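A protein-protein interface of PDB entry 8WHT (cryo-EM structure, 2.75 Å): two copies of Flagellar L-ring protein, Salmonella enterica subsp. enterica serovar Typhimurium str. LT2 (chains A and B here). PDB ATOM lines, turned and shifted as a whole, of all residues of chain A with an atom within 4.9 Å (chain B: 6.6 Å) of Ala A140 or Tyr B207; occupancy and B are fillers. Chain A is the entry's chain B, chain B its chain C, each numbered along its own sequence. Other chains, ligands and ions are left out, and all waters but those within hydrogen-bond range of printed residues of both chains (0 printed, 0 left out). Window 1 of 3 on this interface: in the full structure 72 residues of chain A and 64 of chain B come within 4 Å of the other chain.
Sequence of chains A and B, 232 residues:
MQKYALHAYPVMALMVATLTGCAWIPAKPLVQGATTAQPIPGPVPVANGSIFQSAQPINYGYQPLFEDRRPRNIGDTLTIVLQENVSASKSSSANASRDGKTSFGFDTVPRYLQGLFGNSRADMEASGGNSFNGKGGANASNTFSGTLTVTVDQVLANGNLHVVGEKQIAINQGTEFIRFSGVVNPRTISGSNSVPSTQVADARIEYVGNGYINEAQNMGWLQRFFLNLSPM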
ATOM      1  N   VAL A  86      18.541 -13.520  -6.184  1.00  0.00           N
ATOM      2  CA  VAL A  86      18.606 -12.624  -7.333  1.00  0.00           C
ATOM      3  C   VAL A  86      17.272 -12.688  -8.063  1.00  0.00           C
ATOM      4  O   VAL A  86      16.717 -13.775  -8.251  1.00  0.00           O
ATOM      5  CB  VAL A  86      19.768 -12.983  -8.275  1.00  0.00           C
ATOM      6  CG1 VAL A  86      19.906 -11.941  -9.371  1.00  0.00           C
ATOM      7  CG2 VAL A  86      21.061 -13.107  -7.493  1.00  0.00           C
ATOM      8  N   SER A  87      16.757 -11.525  -8.458  1.00  0.00           N
ATOM      9  CA  SER A  87      15.467 -11.447  -9.138  1.00  0.00           C
ATOM     10  C   SER A  87      15.473 -10.221 -10.038  1.00  0.00           C
ATOM     11  O   SER A  87      15.607  -9.096  -9.551  1.00  0.00           O
ATOM     12  CB  SER A  87      14.322 -11.382  -8.132  1.00  0.00           C
ATOM     13  OG  SER A  87      13.090 -11.732  -8.737  1.00  0.00           O
ATOM     14  N   ALA A  88      15.327 -10.436 -11.343  1.00  0.00           N
ATOM     15  CA  ALA A  88      15.241  -9.359 -12.314  1.00  0.00           C
ATOM     16  C   ALA A  88      13.997  -9.543 -13.172  1.00  0.00           C
ATOM     17  O   ALA A  88      13.565 -10.670 -13.429  1.00  0.00           O
ATOM     18  CB  ALA A  88      16.487  -9.304 -13.202  1.00  0.00           C
ATOM     19  N   ALA A 138      10.028 -10.267 -19.734  1.00  0.00           N
ATOM     20  CA  ALA A 138      10.881 -11.371 -19.320  1.00  0.00           C
ATOM     21  C   ALA A 138      11.186 -11.212 -17.841  1.00  0.00           C
ATOM     22  O   ALA A 138      11.046 -10.122 -17.280  1.00  0.00           O
ATOM     23  CB  ALA A 138      12.175 -11.426 -20.137  1.00  0.00           C
ATOM     24  N   ASN A 139      11.583 -12.311 -17.211  1.00  0.00           N
ATOM     25  CA  ASN A 139      11.942 -12.279 -15.802  1.00  0.00           C
ATOM     26  C   ASN A 139      12.760 -13.515 -15.470  1.00  0.00           C
ATOM     27  O   ASN A 139      12.550 -14.587 -16.039  1.00  0.00           O
ATOM     28  CB  ASN A 139      10.701 -12.198 -14.902  1.00  0.00           C
ATOM     29  CG  ASN A 139       9.832 -13.433 -14.993  1.00  0.00           C
ATOM     30  OD1 ASN A 139       8.912 -13.498 -15.807  1.00  0.00           O
ATOM     31  ND2 ASN A 139      10.109 -14.417 -14.147  1.00  0.00           N
ATOM     32  N   ALA A 140      13.696 -13.343 -14.544  1.00  0.00           N
ATOM     33  CA  ALA A 140      14.535 -14.432 -14.072  1.00  0.00           C
ATOM     34  C   ALA A 140      14.741 -14.283 -12.574  1.00  0.00           C
ATOM     35  O   ALA A 140      14.685 -13.180 -12.030  1.00  0.00           O
ATOM     36  CB  ALA A 140      15.887 -14.461 -14.794  1.00  0.00           C
ATOM     37  N   SER A 141      14.967 -15.413 -11.909  1.00  0.00           N
ATOM     38  CA  SER A 141      15.220 -15.406 -10.478  1.00  0.00           C
ATOM     39  C   SER A 141      15.995 -16.657 -10.105  1.00  0.00           C
ATOM     40  O   SER A 141      15.957 -17.671 -10.807  1.00  0.00           O
ATOM     41  CB  SER A 141      13.919 -15.324  -9.675  1.00  0.00           C
ATOM     42  OG  SER A 141      13.407 -16.618  -9.403  1.00  0.00           O
ATOM     43  N   ASN A 142      16.706 -16.570  -8.986  1.00  0.00           N
ATOM     44  CA  ASN A 142      17.425 -17.716  -8.448  1.00  0.00           C
ATOM     45  C   ASN A 142      17.678 -17.499  -6.965  1.00  0.00           C
ATOM     46  O   ASN A 142      17.987 -16.386  -6.522  1.00  0.00           O
ATOM     47  CB  ASN A 142      18.741 -17.968  -9.201  1.00  0.00           C
ATOM     48  CG  ASN A 142      19.854 -17.032  -8.778  1.00  0.00           C
ATOM     49  OD1 ASN A 142      20.513 -17.247  -7.760  1.00  0.00           O
ATOM     50  ND2 ASN A 142      20.079 -15.989  -9.567  1.00  0.00           N
ATOM     51  N   PHE B 144      15.638  -4.970 -10.951  1.00  0.00           N
ATOM     52  CA  PHE B 144      16.757  -5.866 -10.703  1.00  0.00           C
ATOM     53  C   PHE B 144      17.116  -5.790  -9.230  1.00  0.00           C
ATOM     54  O   PHE B 144      17.269  -4.696  -8.683  1.00  0.00           O
ATOM     55  CB  PHE B 144      17.973  -5.504 -11.566  1.00  0.00           C
ATOM     56  CG  PHE B 144      18.826  -6.682 -11.938  1.00  0.00           C
ATOM     57  CD1 PHE B 144      19.463  -7.430 -10.964  1.00  0.00           C
ATOM     58  CD2 PHE B 144      18.999  -7.035 -13.265  1.00  0.00           C
ATOM     59  CE1 PHE B 144      20.251  -8.513 -11.304  1.00  0.00           C
ATOM     60  CE2 PHE B 144      19.786  -8.116 -13.612  1.00  0.00           C
ATOM     61  CZ  PHE B 144      20.413  -8.855 -12.629  1.00  0.00           C
ATOM     62  N   GLU B 176      23.371 -20.370 -14.827  1.00  0.00           N
ATOM     63  CA  GLU B 176      23.029 -18.961 -14.906  1.00  0.00           C
ATOM     64  C   GLU B 176      24.264 -18.110 -14.643  1.00  0.00           C
ATOM     65  O   GLU B 176      25.091 -18.432 -13.784  1.00  0.00           O
ATOM     66  CB  GLU B 176      21.930 -18.602 -13.902  1.00  0.00           C
ATOM     67  CG  GLU B 176      20.732 -19.534 -13.933  1.00  0.00           C
ATOM     68  CD  GLU B 176      19.421 -18.793 -14.096  1.00  0.00           C
ATOM     69  OE1 GLU B 176      18.828 -18.396 -13.071  1.00  0.00           O
ATOM     70  OE2 GLU B 176      18.981 -18.611 -15.250  1.00  0.00           O
ATOM     71  N   PHE B 177      24.375 -17.021 -15.397  1.00  0.00           N
ATOM     72  CA  PHE B 177      25.483 -16.082 -15.295  1.00  0.00           C
ATOM     73  C   PHE B 177      24.937 -14.698 -14.981  1.00  0.00           C
ATOM     74  O   PHE B 177      24.009 -14.224 -15.648  1.00  0.00           O
ATOM     75  CB  PHE B 177      26.302 -16.026 -16.591  1.00  0.00           C
ATOM     76  CG  PHE B 177      26.544 -17.368 -17.222  1.00  0.00           C
ATOM     77  CD1 PHE B 177      25.584 -17.957 -18.027  1.00  0.00           C
ATOM     78  CD2 PHE B 177      27.741 -18.032 -17.021  1.00  0.00           C
ATOM     79  CE1 PHE B 177      25.810 -19.186 -18.607  1.00  0.00           C
ATOM     80  CE2 PHE B 177      27.972 -19.261 -17.600  1.00  0.00           C
ATOM     81  CZ  PHE B 177      27.006 -19.838 -18.393  1.00  0.00           C
ATOM     82  N   ILE B 178      25.514 -14.061 -13.965  1.00  0.00           N
ATOM     83  CA  ILE B 178      25.242 -12.669 -13.630  1.00  0.00           C
ATOM     84  C   ILE B 178      26.552 -11.915 -13.787  1.00  0.00           C
ATOM     85  O   ILE B 178      27.500 -12.143 -13.025  1.00  0.00           O
ATOM     86  CB  ILE B 178      24.684 -12.510 -12.209  1.00  0.00           C
ATOM     87  CG1 ILE B 178      23.390 -13.307 -12.043  1.00  0.00           C
ATOM     88  CG2 ILE B 178      24.443 -11.043 -11.898  1.00  0.00           C
ATOM     89  CD1 ILE B 178      23.544 -14.551 -11.203  1.00  0.00           C
ATOM     90  N   ARG B 179      26.612 -11.017 -14.764  1.00  0.00           N
ATOM     91  CA  ARG B 179      27.810 -10.239 -15.039  1.00  0.00           C
ATOM     92  C   ARG B 179      27.548  -8.760 -14.789  1.00  0.00           C
ATOM     93  O   ARG B 179      26.479  -8.238 -15.109  1.00  0.00           O
ATOM     94  CB  ARG B 179      28.290 -10.438 -16.480  1.00  0.00           C
ATOM     95  CG  ARG B 179      29.033 -11.738 -16.710  1.00  0.00           C
ATOM     96  CD  ARG B 179      29.466 -11.880 -18.156  1.00  0.00           C
ATOM     97  NE  ARG B 179      28.417 -12.458 -18.984  1.00  0.00           N
ATOM     98  CZ  ARG B 179      28.359 -13.736 -19.336  1.00  0.00           C
ATOM     99  NH1 ARG B 179      29.280 -14.603 -18.946  1.00  0.00           N
ATOM    100  NH2 ARG B 179      27.354 -14.153 -20.100  1.00  0.00           N
ATOM    101  N   ILE B 205      24.839  -4.552 -16.841  1.00  0.00           N
ATOM    102  CA  ILE B 205      24.281  -5.625 -16.025  1.00  0.00           C
ATOM    103  C   ILE B 205      23.709  -6.684 -16.955  1.00  0.00           C
ATOM    104  O   ILE B 205      22.939  -6.367 -17.868  1.00  0.00           O
ATOM    105  CB  ILE B 205      23.203  -5.099 -15.062  1.00  0.00           C
ATOM    106  CG1 ILE B 205      23.662  -3.792 -14.413  1.00  0.00           C
ATOM    107  CG2 ILE B 205      22.880  -6.138 -14.004  1.00  0.00           C
ATOM    108  CD1 ILE B 205      22.644  -3.185 -13.475  1.00  0.00           C
ATOM    109  N   GLU B 206      24.084  -7.940 -16.723  1.00  0.00           N
ATOM    110  CA  GLU B 206      23.640  -9.046 -17.556  1.00  0.00           C
ATOM    111  C   GLU B 206      23.232 -10.211 -16.667  1.00  0.00           C
ATOM    112  O   GLU B 206      23.925 -10.533 -15.701  1.00  0.00           O
ATOM    113  CB  GLU B 206      24.744  -9.480 -18.528  1.00  0.00           C
ATOM    114  CG  GLU B 206      24.464 -10.770 -19.271  1.00  0.00           C
ATOM    115  CD  GLU B 206      25.319 -10.917 -20.514  1.00  0.00           C
ATOM    116  OE1 GLU B 206      26.333 -10.199 -20.622  1.00  0.00           O
ATOM    117  OE2 GLU B 206      24.977 -11.748 -21.382  1.00  0.00           O
ATOM    118  N   TYR B 207      22.106 -10.841 -17.004  1.00  0.00           N
ATOM    119  CA  TYR B 207      21.606 -11.992 -16.252  1.00  0.00           C
ATOM    120  C   TYR B 207      21.035 -12.968 -17.278  1.00  0.00           C
ATOM    121  O   TYR B 207      19.913 -12.779 -17.755  1.00  0.00           O
ATOM    122  CB  TYR B 207      20.561 -11.566 -15.227  1.00  0.00           C
ATOM    123  CG  TYR B 207      20.065 -12.670 -14.317  1.00  0.00           C
ATOM    124  CD1 TYR B 207      20.712 -13.897 -14.249  1.00  0.00           C
ATOM    125  CD2 TYR B 207      18.946 -12.480 -13.519  1.00  0.00           C
ATOM    126  CE1 TYR B 207      20.258 -14.900 -13.420  1.00  0.00           C
ATOM    127  CE2 TYR B 207      18.484 -13.479 -12.684  1.00  0.00           C
ATOM    128  CZ  TYR B 207      19.144 -14.686 -12.640  1.00  0.00           C
ATOM    129  OH  TYR B 207      18.687 -15.679 -11.809  1.00  0.00           O
ATOM    130  N   VAL B 208      21.807 -14.001 -17.608  1.00  0.00           N
ATOM    131  CA  VAL B 208      21.454 -14.938 -18.665  1.00  0.00           C
ATOM    132  C   VAL B 208      21.611 -16.364 -18.144  1.00  0.00           C
ATOM    133  O   VAL B 208      22.052 -16.589 -17.019  1.00  0.00           O
ATOM    134  CB  VAL B 208      22.294 -14.724 -19.941  1.00  0.00           C
ATOM    135  CG1 VAL B 208      22.115 -13.312 -20.467  1.00  0.00           C
ATOM    136  CG2 VAL B 208      23.758 -15.011 -19.664  1.00  0.00           C
ATOM    137  N   GLY B 209      21.227 -17.332 -18.978  1.00  0.00           N
ATOM    138  CA  GLY B 209      21.350 -18.731 -18.623  1.00  0.00           C
ATOM    139  C   GLY B 209      21.420 -19.607 -19.855  1.00  0.00           C
ATOM    140  O   GLY B 209      21.226 -19.151 -20.982  1.00  0.00           O
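Tyr B207 touches just these residues of chain A: Val A86 (3.9 Å), Ala A140 (3.5 Å), Ser A141 (3.3 Å) and Asn A142 (2.7 Å).
Of the printed residues of chain B, Asn A142 touches Glu B176 and Tyr B207.
Of the printed residues of chain A, Phe B144 touches Val A86 (3.95 Å), Ser A87 (3.6 Å) and Ala A88 (3.4 Å).
Ile B205 touches none of the printed residues of chain A.
Ile B178 touches none of the printed residues of chain A.
The nearest residue of chain A that does not touch Tyr B207 is Ala A88 (4.03 Å).
Val A86 touches Phe B144.
Tyr B207 touches Val A86 (CE2 to CG1, 3.9 Å).
Ser A87 touches Phe B144 (O to CA, 3.6 Å).
Ala A88 touches Phe B144 (CB to CD2, 3.4 Å).
Ala A140 touches Tyr B207 (CB to CE2, 3.5 Å).
O of Ser A141 touches OE1 of Glu B176, 3.7 Å away.
C of Ser A141 touches OH of Tyr B207, at 3.3 Å.
Asn A142 touches Glu B176.
No position is printed for both chains.
Of the 9 pairs that touch across the chains among the printed residues, none has its exchanged pair printed and touching as well.
Of the 8 printed residues of chain A, 6 touch a printed residue of chain B.
Printed residues of chain A that touch a printed residue of chain B: Val A86, Ser A87, Ala A88, Ala A140, Ser A141 and Asn A142.
Hydrophobic or aromatic side chains of chain A within 4 Å of the printed part of chain B: Val A86, Ala A88 and Ala A140.
Of the 10 printed residues of chain B, 3 touch a printed residue of chain A.
Hydrophobic or aromatic side chains of chain B within 4 Å of the printed part of chain A: Phe B144 and Tyr B207.
Among the printed residues, 9 pairs touch across the chains.
Among the printed residues, no Asp or Glu carboxylate lies within 4 Å of a Lys or Arg side-chain nitrogen of the other chain.
The side-chain hydroxyl of Tyr B207 is in hydrogen-bond range of the side-chain amide nitrogen of Asn A142.
The backbone NH (N) of Asn A142 is in hydrogen-bond range of the backbone carbonyl oxygen (O) of Val A86, 2.9 Å away.
The side-chain carboxylate (OE1) of Glu B176 sits at hydrogen-bond distance from the side-chain hydroxyl (OH) of Tyr B207.
O of Ala A88 lies within hydrogen-bond range of N of Ala A140, at 2.9 Å.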
